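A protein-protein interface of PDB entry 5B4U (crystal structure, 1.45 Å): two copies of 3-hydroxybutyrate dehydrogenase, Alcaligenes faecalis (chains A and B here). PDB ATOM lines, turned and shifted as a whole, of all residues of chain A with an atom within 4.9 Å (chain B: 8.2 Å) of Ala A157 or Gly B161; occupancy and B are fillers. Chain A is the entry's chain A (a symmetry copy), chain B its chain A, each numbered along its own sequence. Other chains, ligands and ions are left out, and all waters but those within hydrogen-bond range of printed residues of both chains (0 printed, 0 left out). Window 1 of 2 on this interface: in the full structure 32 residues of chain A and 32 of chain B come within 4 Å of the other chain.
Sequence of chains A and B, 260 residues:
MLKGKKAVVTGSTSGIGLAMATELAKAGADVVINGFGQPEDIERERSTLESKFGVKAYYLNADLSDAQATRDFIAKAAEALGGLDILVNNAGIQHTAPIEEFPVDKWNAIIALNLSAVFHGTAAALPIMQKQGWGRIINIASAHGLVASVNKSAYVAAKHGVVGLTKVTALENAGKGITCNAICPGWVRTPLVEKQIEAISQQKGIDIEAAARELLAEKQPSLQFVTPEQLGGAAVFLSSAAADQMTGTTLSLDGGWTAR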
ATOM      1  N   TRP A 107       2.003  -9.536   1.020  1.00  0.00           N
ATOM      2  CA  TRP A 107       1.377  -9.533  -0.298  1.00  0.00           C
ATOM      3  C   TRP A 107       1.903 -10.694  -1.125  1.00  0.00           C
ATOM      4  O   TRP A 107       1.133 -11.502  -1.627  1.00  0.00           O
ATOM      5  CB  TRP A 107       1.615  -8.205  -1.019  1.00  0.00           C
ATOM      6  CG  TRP A 107       1.247  -8.231  -2.475  1.00  0.00           C
ATOM      7  CD1 TRP A 107       2.047  -8.607  -3.509  1.00  0.00           C
ATOM      8  CD2 TRP A 107      -0.021  -7.893  -3.057  1.00  0.00           C
ATOM      9  NE1 TRP A 107       1.336  -8.614  -4.684  1.00  0.00           N
ATOM     10  CE2 TRP A 107       0.059  -8.190  -4.431  1.00  0.00           C
ATOM     11  CE3 TRP A 107      -1.219  -7.378  -2.549  1.00  0.00           C
ATOM     12  CZ2 TRP A 107      -1.012  -7.995  -5.302  1.00  0.00           C
ATOM     13  CZ3 TRP A 107      -2.287  -7.203  -3.420  1.00  0.00           C
ATOM     14  CH2 TRP A 107      -2.174  -7.517  -4.775  1.00  0.00           C
ATOM     15  N   ILE A 111      -0.419 -13.911  -2.319  1.00  0.00           N
ATOM     16  CA  ILE A 111      -0.558 -14.193  -3.741  1.00  0.00           C
ATOM     17  C   ILE A 111       0.014 -15.572  -4.079  1.00  0.00           C
ATOM     18  O   ILE A 111      -0.616 -16.355  -4.796  1.00  0.00           O
ATOM     19  CB  ILE A 111       0.108 -13.104  -4.603  1.00  0.00           C
ATOM     20  CG1 ILE A 111      -0.600 -11.756  -4.424  1.00  0.00           C
ATOM     21  CG2 ILE A 111       0.125 -13.512  -6.067  1.00  0.00           C
ATOM     22  CD1 ILE A 111      -2.072 -11.770  -4.771  1.00  0.00           C
ATOM     23  N   LYS A 152      -7.803  -5.916   3.558  1.00  0.00           N
ATOM     24  CA  LYS A 152      -7.570  -7.247   3.018  1.00  0.00           C
ATOM     25  C   LYS A 152      -7.215  -7.206   1.538  1.00  0.00           C
ATOM     26  O   LYS A 152      -7.608  -8.081   0.771  1.00  0.00           O
ATOM     27  CB  LYS A 152      -8.797  -8.124   3.259  1.00  0.00           C
ATOM     28  CG  LYS A 152      -8.977  -8.471   4.727  1.00  0.00           C
ATOM     29  CD  LYS A 152     -10.195  -9.340   4.982  1.00  0.00           C
ATOM     30  CE  LYS A 152     -10.254  -9.746   6.446  1.00  0.00           C
ATOM     31  NZ  LYS A 152     -11.413 -10.627   6.748  1.00  0.00           N
ATOM     32  N   SER A 153      -6.374  -6.252   1.156  1.00  0.00           N
ATOM     33  CA  SER A 153      -6.034  -6.078  -0.250  1.00  0.00           C
ATOM     34  C   SER A 153      -5.515  -7.365  -0.888  1.00  0.00           C
ATOM     35  O   SER A 153      -5.993  -7.783  -1.944  1.00  0.00           O
ATOM     36  CB  SER A 153      -5.023  -4.945  -0.430  1.00  0.00           C
ATOM     37  OG  SER A 153      -3.879  -5.113   0.396  1.00  0.00           O
ATOM     38  N   ALA A 154      -4.472  -7.950  -0.310  1.00  0.00           N
ATOM     39  CA  ALA A 154      -3.856  -9.122  -0.918  1.00  0.00           C
ATOM     40  C   ALA A 154      -4.854 -10.275  -1.017  1.00  0.00           C
ATOM     41  O   ALA A 154      -4.886 -11.000  -2.012  1.00  0.00           O
ATOM     42  CB  ALA A 154      -2.619  -9.540  -0.132  1.00  0.00           C
ATOM     43  N   TYR A 155      -5.582 -10.505   0.067  1.00  0.00           N
ATOM     44  CA  TYR A 155      -6.487 -11.636   0.156  1.00  0.00           C
ATOM     45  C   TYR A 155      -7.656 -11.492  -0.822  1.00  0.00           C
ATOM     46  O   TYR A 155      -7.980 -12.422  -1.554  1.00  0.00           O
ATOM     47  CB  TYR A 155      -7.006 -11.752   1.590  1.00  0.00           C
ATOM     48  CG  TYR A 155      -7.852 -12.974   1.847  1.00  0.00           C
ATOM     49  CD1 TYR A 155      -7.275 -14.152   2.287  1.00  0.00           C
ATOM     50  CD2 TYR A 155      -9.235 -12.907   1.794  1.00  0.00           C
ATOM     51  CE1 TYR A 155      -8.047 -15.221   2.691  1.00  0.00           C
ATOM     52  CE2 TYR A 155     -10.013 -13.996   2.122  1.00  0.00           C
ATOM     53  CZ  TYR A 155      -9.416 -15.130   2.620  1.00  0.00           C
ATOM     54  OH  TYR A 155     -10.187 -16.194   3.016  1.00  0.00           O
ATOM     55  N   VAL A 156      -8.256 -10.310  -0.863  1.00  0.00           N
ATOM     56  CA  VAL A 156      -9.337 -10.044  -1.807  1.00  0.00           C
ATOM     57  C   VAL A 156      -8.851 -10.139  -3.248  1.00  0.00           C
ATOM     58  O   VAL A 156      -9.508 -10.739  -4.097  1.00  0.00           O
ATOM     59  CB  VAL A 156      -9.975  -8.665  -1.552  1.00  0.00           C
ATOM     60  CG1 VAL A 156     -10.966  -8.314  -2.651  1.00  0.00           C
ATOM     61  CG2 VAL A 156     -10.662  -8.647  -0.200  1.00  0.00           C
ATOM     62  N   ALA A 157      -7.675  -9.588  -3.529  1.00  0.00           N
ATOM     63  CA  ALA A 157      -7.100  -9.710  -4.861  1.00  0.00           C
ATOM     64  C   ALA A 157      -6.899 -11.183  -5.225  1.00  0.00           C
ATOM     65  O   ALA A 157      -7.267 -11.626  -6.318  1.00  0.00           O
ATOM     66  CB  ALA A 157      -5.787  -8.952  -4.950  1.00  0.00           C
ATOM     67  N   ALA A 158      -6.283 -11.935  -4.322  1.00  0.00           N
ATOM     68  CA  ALA A 158      -6.023 -13.343  -4.571  1.00  0.00           C
ATOM     69  C   ALA A 158      -7.308 -14.122  -4.819  1.00  0.00           C
ATOM     70  O   ALA A 158      -7.373 -14.939  -5.731  1.00  0.00           O
ATOM     71  CB  ALA A 158      -5.256 -13.952  -3.411  1.00  0.00           C
ATOM     72  N   LYS A 159      -8.321 -13.887  -3.987  1.00  0.00           N
ATOM     73  CA  LYS A 159      -9.557 -14.655  -4.067  1.00  0.00           C
ATOM     74  C   LYS A 159     -10.377 -14.277  -5.298  1.00  0.00           C
ATOM     75  O   LYS A 159     -10.959 -15.144  -5.940  1.00  0.00           O
ATOM     76  CB  LYS A 159     -10.399 -14.488  -2.796  1.00  0.00           C
ATOM     77  CG  LYS A 159      -9.764 -15.077  -1.545  1.00  0.00           C
ATOM     78  CD  LYS A 159      -9.574 -16.580  -1.664  1.00  0.00           C
ATOM     79  CE  LYS A 159      -9.240 -17.218  -0.323  1.00  0.00           C
ATOM     80  NZ  LYS A 159      -9.063 -18.689  -0.436  1.00  0.00           N
ATOM     81  N   HIS A 160     -10.374 -13.000  -5.668  1.00  0.00           N
ATOM     82  CA  HIS A 160     -10.939 -12.595  -6.953  1.00  0.00           C
ATOM     83  C   HIS A 160     -10.194 -13.305  -8.081  1.00  0.00           C
ATOM     84  O   HIS A 160     -10.809 -13.859  -8.991  1.00  0.00           O
ATOM     85  CB  HIS A 160     -10.851 -11.079  -7.143  1.00  0.00           C
ATOM     86  CG  HIS A 160     -12.016 -10.327  -6.575  1.00  0.00           C
ATOM     87  ND1 HIS A 160     -12.269 -10.258  -5.221  1.00  0.00           N
ATOM     88  CD2 HIS A 160     -12.971  -9.577  -7.172  1.00  0.00           C
ATOM     89  CE1 HIS A 160     -13.344  -9.519  -5.013  1.00  0.00           C
ATOM     90  NE2 HIS A 160     -13.798  -9.108  -6.182  1.00  0.00           N
ATOM     91  N   GLY A 161      -8.874 -13.397  -7.950  1.00  0.00           N
ATOM     92  CA  GLY A 161      -8.056 -14.111  -8.924  1.00  0.00           C
ATOM     93  C   GLY A 161      -8.435 -15.569  -9.060  1.00  0.00           C
ATOM     94  O   GLY A 161      -8.504 -16.101 -10.167  1.00  0.00           O
ATOM     95  N   ILE B 111       1.273 -11.821 -13.436  1.00  0.00           N
ATOM     96  CA  ILE B 111       0.865 -11.467 -12.084  1.00  0.00           C
ATOM     97  C   ILE B 111       1.668 -10.269 -11.571  1.00  0.00           C
ATOM     98  O   ILE B 111       1.102  -9.328 -11.006  1.00  0.00           O
ATOM     99  CB  ILE B 111       0.996 -12.661 -11.121  1.00  0.00           C
ATOM    100  CG1 ILE B 111       0.034 -13.788 -11.513  1.00  0.00           C
ATOM    101  CG2 ILE B 111       0.756 -12.223  -9.684  1.00  0.00           C
ATOM    102  CD1 ILE B 111      -1.424 -13.387 -11.538  1.00  0.00           C
ATOM    103  N   ASN B 114       0.575  -7.059 -14.094  1.00  0.00           N
ATOM    104  CA  ASN B 114      -0.842  -6.767 -14.265  1.00  0.00           C
ATOM    105  C   ASN B 114      -1.589  -6.678 -12.933  1.00  0.00           C
ATOM    106  O   ASN B 114      -2.679  -6.117 -12.875  1.00  0.00           O
ATOM    107  CB  ASN B 114      -1.510  -7.826 -15.143  1.00  0.00           C
ATOM    108  CG  ASN B 114      -1.055  -7.773 -16.592  1.00  0.00           C
ATOM    109  OD1 ASN B 114       0.055  -7.340 -16.898  1.00  0.00           O
ATOM    110  ND2 ASN B 114      -1.895  -8.282 -17.487  1.00  0.00           N
ATOM    111  N   LEU B 115      -1.051  -7.299 -11.889  1.00  0.00           N
ATOM    112  CA  LEU B 115      -1.690  -7.250 -10.576  1.00  0.00           C
ATOM    113  C   LEU B 115      -0.794  -6.589  -9.531  1.00  0.00           C
ATOM    114  O   LEU B 115      -1.163  -5.586  -8.939  1.00  0.00           O
ATOM    115  CB  LEU B 115      -2.126  -8.647 -10.127  1.00  0.00           C
ATOM    116  CG  LEU B 115      -2.761  -8.751  -8.740  1.00  0.00           C
ATOM    117  CD1 LEU B 115      -3.968  -7.833  -8.614  1.00  0.00           C
ATOM    118  CD2 LEU B 115      -3.138 -10.193  -8.440  1.00  0.00           C
ATOM    119  N   SER B 116       0.376  -7.155  -9.278  1.00  0.00           N
ATOM    120  CA  SER B 116       1.173  -6.671  -8.163  1.00  0.00           C
ATOM    121  C   SER B 116       1.602  -5.216  -8.334  1.00  0.00           C
ATOM    122  O   SER B 116       1.605  -4.461  -7.370  1.00  0.00           O
ATOM    123  CB  SER B 116       2.380  -7.569  -7.946  1.00  0.00           C
ATOM    124  OG  SER B 116       1.952  -8.856  -7.542  1.00  0.00           O
ATOM    125  N   VAL B 118      -0.059  -2.867  -9.562  1.00  0.00           N
ATOM    126  CA  VAL B 118      -1.193  -2.043  -9.193  1.00  0.00           C
ATOM    127  C   VAL B 118      -1.247  -1.845  -7.680  1.00  0.00           C
ATOM    128  O   VAL B 118      -1.379  -0.720  -7.195  1.00  0.00           O
ATOM    129  CB  VAL B 118      -2.513  -2.661  -9.682  1.00  0.00           C
ATOM    130  CG1 VAL B 118      -3.683  -1.765  -9.312  1.00  0.00           C
ATOM    131  CG2 VAL B 118      -2.461  -2.883 -11.184  1.00  0.00           C
ATOM    132  N   PHE B 119      -0.966  -2.913  -6.941  1.00  0.00           N
ATOM    133  CA  PHE B 119      -0.851  -2.834  -5.494  1.00  0.00           C
ATOM    134  C   PHE B 119       0.293  -1.912  -5.070  1.00  0.00           C
ATOM    135  O   PHE B 119       0.104  -1.008  -4.254  1.00  0.00           O
ATOM    136  CB  PHE B 119      -0.666  -4.231  -4.900  1.00  0.00           C
ATOM    137  CG  PHE B 119      -0.175  -4.223  -3.487  1.00  0.00           C
ATOM    138  CD1 PHE B 119      -1.024  -3.901  -2.441  1.00  0.00           C
ATOM    139  CD2 PHE B 119       1.115  -4.622  -3.198  1.00  0.00           C
ATOM    140  CE1 PHE B 119      -0.574  -3.951  -1.131  1.00  0.00           C
ATOM    141  CE2 PHE B 119       1.578  -4.638  -1.897  1.00  0.00           C
ATOM    142  CZ  PHE B 119       0.733  -4.297  -0.864  1.00  0.00           C
ATOM    143  N   ASN B 139      -7.665   2.159 -12.264  1.00  0.00           N
ATOM    144  CA  ASN B 139      -7.026   0.911 -12.650  1.00  0.00           C
ATOM    145  C   ASN B 139      -7.595   0.431 -13.976  1.00  0.00           C
ATOM    146  O   ASN B 139      -8.802   0.433 -14.172  1.00  0.00           O
ATOM    147  CB  ASN B 139      -7.254  -0.150 -11.569  1.00  0.00           C
ATOM    148  CG  ASN B 139      -6.611   0.218 -10.249  1.00  0.00           C
ATOM    149  OD1 ASN B 139      -7.096  -0.153  -9.171  1.00  0.00           O
ATOM    150  ND2 ASN B 139      -5.499   0.921 -10.323  1.00  0.00           N
ATOM    151  N   ALA B 141      -8.418  -2.491 -15.847  1.00  0.00           N
ATOM    152  CA  ALA B 141      -8.620  -3.924 -15.803  1.00  0.00           C
ATOM    153  C   ALA B 141      -8.970  -4.413 -17.203  1.00  0.00           C
ATOM    154  O   ALA B 141      -8.192  -4.208 -18.135  1.00  0.00           O
ATOM    155  CB  ALA B 141      -9.697  -4.283 -14.794  1.00  0.00           C
ATOM    156  N   HIS B 144     -12.058  -9.052 -18.918  1.00  0.00           N
ATOM    157  CA  HIS B 144     -11.485 -10.267 -18.347  1.00  0.00           C
ATOM    158  C   HIS B 144     -11.165 -10.132 -16.862  1.00  0.00           C
ATOM    159  O   HIS B 144     -10.685 -11.083 -16.246  1.00  0.00           O
ATOM    160  CB  HIS B 144     -10.215 -10.650 -19.108  1.00  0.00           C
ATOM    161  CG  HIS B 144     -10.485 -11.361 -20.394  1.00  0.00           C
ATOM    162  ND1 HIS B 144      -9.978 -10.928 -21.600  1.00  0.00           N
ATOM    163  CD2 HIS B 144     -11.385 -12.324 -20.695  1.00  0.00           C
ATOM    164  CE1 HIS B 144     -10.427 -11.710 -22.565  1.00  0.00           C
ATOM    165  NE2 HIS B 144     -11.301 -12.551 -22.046  1.00  0.00           N
ATOM    166  N   GLY B 145     -11.541  -9.005 -16.267  1.00  0.00           N
ATOM    167  CA  GLY B 145     -11.643  -8.895 -14.819  1.00  0.00           C
ATOM    168  C   GLY B 145     -13.004  -9.289 -14.279  1.00  0.00           C
ATOM    169  O   GLY B 145     -13.189  -9.351 -13.066  1.00  0.00           O
ATOM    170  N   LEU B 146     -13.956  -9.531 -15.185  1.00  0.00           N
ATOM    171  CA  LEU B 146     -15.338  -9.855 -14.815  1.00  0.00           C
ATOM    172  C   LEU B 146     -15.775 -11.220 -15.347  1.00  0.00           C
ATOM    173  O   LEU B 146     -16.612 -11.889 -14.739  1.00  0.00           O
ATOM    174  CB  LEU B 146     -16.289  -8.773 -15.338  1.00  0.00           C
ATOM    175  CG  LEU B 146     -15.982  -7.356 -14.847  1.00  0.00           C
ATOM    176  CD1 LEU B 146     -16.824  -6.327 -15.591  1.00  0.00           C
ATOM    177  CD2 LEU B 146     -16.207  -7.256 -13.347  1.00  0.00           C
ATOM    178  N   ALA B 154      -3.544 -16.611 -16.575  1.00  0.00           N
ATOM    179  CA  ALA B 154      -2.819 -15.616 -15.796  1.00  0.00           C
ATOM    180  C   ALA B 154      -3.481 -14.244 -15.908  1.00  0.00           C
ATOM    181  O   ALA B 154      -3.571 -13.502 -14.929  1.00  0.00           O
ATOM    182  CB  ALA B 154      -1.362 -15.553 -16.239  1.00  0.00           C
ATOM    183  N   TYR B 155      -3.837 -13.871 -17.130  1.00  0.00           N
ATOM    184  CA  TYR B 155      -4.372 -12.549 -17.403  1.00  0.00           C
ATOM    185  C   TYR B 155      -5.742 -12.358 -16.748  1.00  0.00           C
ATOM    186  O   TYR B 155      -5.988 -11.353 -16.089  1.00  0.00           O
ATOM    187  CB  TYR B 155      -4.474 -12.351 -18.915  1.00  0.00           C
ATOM    188  CG  TYR B 155      -4.889 -10.963 -19.334  1.00  0.00           C
ATOM    189  CD1 TYR B 155      -3.940  -9.986 -19.579  1.00  0.00           C
ATOM    190  CD2 TYR B 155      -6.213 -10.673 -19.626  1.00  0.00           C
ATOM    191  CE1 TYR B 155      -4.291  -8.770 -20.126  1.00  0.00           C
ATOM    192  CE2 TYR B 155      -6.582  -9.432 -20.099  1.00  0.00           C
ATOM    193  CZ  TYR B 155      -5.611  -8.505 -20.398  1.00  0.00           C
ATOM    194  OH  TYR B 155      -5.962  -7.293 -20.937  1.00  0.00           O
ATOM    195  N   VAL B 156      -6.616 -13.346 -16.895  1.00  0.00           N
ATOM    196  CA  VAL B 156      -7.927 -13.296 -16.255  1.00  0.00           C
ATOM    197  C   VAL B 156      -7.803 -13.281 -14.736  1.00  0.00           C
ATOM    198  O   VAL B 156      -8.474 -12.507 -14.057  1.00  0.00           O
ATOM    199  CB  VAL B 156      -8.812 -14.474 -16.704  1.00  0.00           C
ATOM    200  CG1 VAL B 156     -10.099 -14.524 -15.896  1.00  0.00           C
ATOM    201  CG2 VAL B 156      -9.126 -14.360 -18.183  1.00  0.00           C
ATOM    202  N   ALA B 157      -6.914 -14.106 -14.193  1.00  0.00           N
ATOM    203  CA  ALA B 157      -6.673 -14.091 -12.756  1.00  0.00           C
ATOM    204  C   ALA B 157      -6.199 -12.707 -12.307  1.00  0.00           C
ATOM    205  O   ALA B 157      -6.698 -12.149 -11.324  1.00  0.00           O
ATOM    206  CB  ALA B 157      -5.661 -15.156 -12.372  1.00  0.00           C
ATOM    207  N   ALA B 158      -5.208 -12.167 -13.005  1.00  0.00           N
ATOM    208  CA  ALA B 158      -4.667 -10.865 -12.654  1.00  0.00           C
ATOM    209  C   ALA B 158      -5.730  -9.776 -12.706  1.00  0.00           C
ATOM    210  O   ALA B 158      -5.807  -8.940 -11.811  1.00  0.00           O
ATOM    211  CB  ALA B 158      -3.508 -10.510 -13.569  1.00  0.00           C
ATOM    212  N   LYS B 159      -6.532  -9.771 -13.769  1.00  0.00           N
ATOM    213  CA  LYS B 159      -7.512  -8.711 -13.971  1.00  0.00           C
ATOM    214  C   LYS B 159      -8.677  -8.826 -12.992  1.00  0.00           C
ATOM    215  O   LYS B 159      -9.159  -7.819 -12.486  1.00  0.00           O
ATOM    216  CB  LYS B 159      -8.028  -8.698 -15.414  1.00  0.00           C
ATOM    217  CG  LYS B 159      -6.975  -8.332 -16.451  1.00  0.00           C
ATOM    218  CD  LYS B 159      -6.443  -6.924 -16.239  1.00  0.00           C
ATOM    219  CE  LYS B 159      -5.638  -6.437 -17.436  1.00  0.00           C
ATOM    220  NZ  LYS B 159      -5.124  -5.057 -17.235  1.00  0.00           N
ATOM    221  N   HIS B 160      -9.092 -10.049 -12.675  1.00  0.00           N
ATOM    222  CA  HIS B 160     -10.041 -10.254 -11.583  1.00  0.00           C
ATOM    223  C   HIS B 160      -9.441  -9.722 -10.283  1.00  0.00           C
ATOM    224  O   HIS B 160     -10.098  -9.000  -9.535  1.00  0.00           O
ATOM    225  CB  HIS B 160     -10.392 -11.735 -11.426  1.00  0.00           C
ATOM    226  CG  HIS B 160     -11.533 -12.183 -12.288  1.00  0.00           C
ATOM    227  ND1 HIS B 160     -11.455 -12.230 -13.664  1.00  0.00           N
ATOM    228  CD2 HIS B 160     -12.765 -12.645 -11.969  1.00  0.00           C
ATOM    229  CE1 HIS B 160     -12.597 -12.676 -14.154  1.00  0.00           C
ATOM    230  NE2 HIS B 160     -13.414 -12.919 -13.147  1.00  0.00           N
ATOM    231  N   GLY B 161      -8.150  -9.975 -10.082  1.00  0.00           N
ATOM    232  CA  GLY B 161      -7.444  -9.462  -8.913  1.00  0.00           C
ATOM    233  C   GLY B 161      -7.459  -7.952  -8.828  1.00  0.00           C
ATOM    234  O   GLY B 161      -7.660  -7.384  -7.755  1.00  0.00           O
ATOM    235  N   VAL B 162      -7.257  -7.295  -9.965  1.00  0.00           N
ATOM    236  CA  VAL B 162      -7.281  -5.841 -10.019  1.00  0.00           C
ATOM    237  C   VAL B 162      -8.656  -5.308  -9.635  1.00  0.00           C
ATOM    238  O   VAL B 162      -8.765  -4.315  -8.927  1.00  0.00           O
ATOM    239  CB  VAL B 162      -6.893  -5.327 -11.416  1.00  0.00           C
ATOM    240  CG1 VAL B 162      -7.197  -3.841 -11.545  1.00  0.00           C
ATOM    241  CG2 VAL B 162      -5.422  -5.599 -11.674  1.00  0.00           C
ATOM    242  N   VAL B 163      -9.706  -5.951 -10.129  1.00  0.00           N
ATOM    243  CA  VAL B 163     -11.059  -5.561  -9.772  1.00  0.00           C
ATOM    244  C   VAL B 163     -11.309  -5.701  -8.265  1.00  0.00           C
ATOM    245  O   VAL B 163     -11.817  -4.780  -7.627  1.00  0.00           O
ATOM    246  CB  VAL B 163     -12.082  -6.379 -10.574  1.00  0.00           C
ATOM    247  CG1 VAL B 163     -13.480  -6.215  -9.999  1.00  0.00           C
ATOM    248  CG2 VAL B 163     -12.041  -5.966 -12.039  1.00  0.00           C
ATOM    249  N   GLY B 164     -10.787  -6.761  -7.658  1.00  0.00           N
ATOM    250  CA  GLY B 164     -10.884  -6.911  -6.208  1.00  0.00           C
ATOM    251  C   GLY B 164     -10.091  -5.854  -5.463  1.00  0.00           C
ATOM    252  O   GLY B 164     -10.567  -5.270  -4.484  1.00  0.00           O
ATOM    253  N   LEU B 165      -8.863  -5.624  -5.913  1.00  0.00           N
ATOM    254  CA  LEU B 165      -7.991  -4.641  -5.289  1.00  0.00           C
ATOM    255  C   LEU B 165      -8.579  -3.234  -5.374  1.00  0.00           C
ATOM    256  O   LEU B 165      -8.496  -2.448  -4.426  1.00  0.00           O
ATOM    257  CB  LEU B 165      -6.620  -4.683  -5.962  1.00  0.00           C
ATOM    258  CG  LEU B 165      -5.568  -3.694  -5.483  1.00  0.00           C
ATOM    259  CD1 LEU B 165      -5.256  -3.884  -4.006  1.00  0.00           C
ATOM    260  CD2 LEU B 165      -4.317  -3.883  -6.325  1.00  0.00           C
ATOM    261  N   THR B 166      -9.226  -2.939  -6.494  1.00  0.00           N
ATOM    262  CA  THR B 166      -9.915  -1.671  -6.685  1.00  0.00           C
ATOM    263  C   THR B 166     -10.970  -1.455  -5.596  1.00  0.00           C
ATOM    264  O   THR B 166     -11.069  -0.375  -5.007  1.00  0.00           O
ATOM    265  CB  THR B 166     -10.579  -1.645  -8.072  1.00  0.00           C
ATOM    266  OG1 THR B 166      -9.564  -1.739  -9.084  1.00  0.00           O
ATOM    267  CG2 THR B 166     -11.390  -0.378  -8.276  1.00  0.00           C
ATOM    268  N   LYS B 167     -11.754  -2.492  -5.326  1.00  0.00           N
ATOM    269  CA  LYS B 167     -12.789  -2.417  -4.302  1.00  0.00           C
ATOM    270  C   LYS B 167     -12.198  -2.154  -2.919  1.00  0.00           C
ATOM    271  O   LYS B 167     -12.695  -1.308  -2.177  1.00  0.00           O
ATOM    272  CB  LYS B 167     -13.613  -3.704  -4.286  1.00  0.00           C
ATOM    273  CG  LYS B 167     -14.388  -3.985  -5.562  1.00  0.00           C
ATOM    274  CD  LYS B 167     -14.986  -5.384  -5.536  1.00  0.00           C
ATOM    275  CE  LYS B 167     -15.380  -5.854  -6.923  1.00  0.00           C
ATOM    276  NZ  LYS B 167     -15.880  -7.254  -6.895  1.00  0.00           N
ATOM    277  N   VAL B 168     -11.127  -2.860  -2.570  1.00  0.00           N
ATOM    278  CA  VAL B 168     -10.491  -2.645  -1.272  1.00  0.00           C
ATOM    279  C   VAL B 168      -9.963  -1.217  -1.152  1.00  0.00           C
ATOM    280  O   VAL B 168     -10.176  -0.550  -0.146  1.00  0.00           O
ATOM    281  CB  VAL B 168      -9.340  -3.638  -1.025  1.00  0.00           C
ATOM    282  CG1 VAL B 168      -8.637  -3.303   0.282  1.00  0.00           C
ATOM    283  CG2 VAL B 168      -9.869  -5.061  -0.983  1.00  0.00           C
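OG of Ser B116 sits at hydrogen-bond distance from NE1 of Trp A107 (2.9 Å).
A ring nitrogen (NE2) of His A160 sits at hydrogen-bond distance from the side-chain amino group of Lys B167 (2.9 Å).
Of chain B, only Gly B161 (3.4 Å) comes within 4 Å of Ala A157.
Of chain A, only Ala A157 (3.4 Å) comes within 4 Å of Gly B161.
No residue of chain B comes within 4 Å of Ala A158.
Of the printed residues of chain A, His B160 touches His A160.
Printed residues of chain B within 4 Å of Ser A153: Phe B119, Leu B165 and Val B168.
Of the printed residues of chain B, Gly A161 touches Ala B157 (3.4 Å).
Of the printed residues of chain A, Leu B115 touches Trp A107.
Of the printed residues of chain A, Phe B119 touches Trp A107 (3.5 Å) and Ser A153 (3.8 Å).
Lys A152 touches none of the printed residues of chain B.
Lys B159 touches none of the printed residues of chain A.
The nearest residue of chain A that does not touch Gly B161 is Gly A161 (4.1 Å).
The backbone carbonyl oxygen (O) of Ile B111 sits at hydrogen-bond distance from the backbone NH (N) of Ser B116 (2.9 Å).
The backbone carbonyl oxygen (O) of His B144 is in hydrogen-bond range of a ring nitrogen (ND1) of His B160 (2.9 Å).
The backbone carbonyl oxygen (O) of Gly B145 sits close to a ring nitrogen (ND1) of His B160 (3.4 Å).
A ring nitrogen (ND1) of His B160 lies within hydrogen-bond range of the backbone carbonyl oxygen (O) of Val B156.
O of Val A156 lies within hydrogen-bond range of ND1 of His A160 (3.0 Å).
Ile B111 touches its own counterpart, Ile A111.
Ala A157 touches Gly B161, and with the chains exchanged Gly A161 touches Ala B157.
His A160 touches its own counterpart, His B160.
9 positions are printed for both chains.
Of the 14 pairs that touch across the chains among the printed residues, 4 have their exchanged pair printed and touching as well.
Leu B115 touches Trp A107 (CG to CZ2, 3.9 Å).
Phe B119 touches Trp A107.
Ile B111 touches Ile A111 (CG2 to CG2, 3.9 Å).
Ser A153 touches Phe B119 (OG to CE1, 3.8 Å).
Ser A153 touches Val B168.
CG1 of Val A156 touches O of Gly B164, at 3.6 Å.
Ala A157 touches Gly B161.
His B160 touches His A160 (O to CB, 3.3 Å).
CA of Gly B164 touches CD2 of His A160 (3.5 Å).
Gly A161 touches Ala B157.
Of the 12 printed residues of chain A, 7 touch a printed residue of chain B.
Of the 26 printed residues of chain B, 11 touch a printed residue of chain A.
Printed residues of chain B that touch a printed residue of chain A: Ile B111, Leu B115, Ser B116, Phe B119, Ala B157, His B160, Gly B161, Gly B164, Leu B165, Lys B167 and Val B168.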
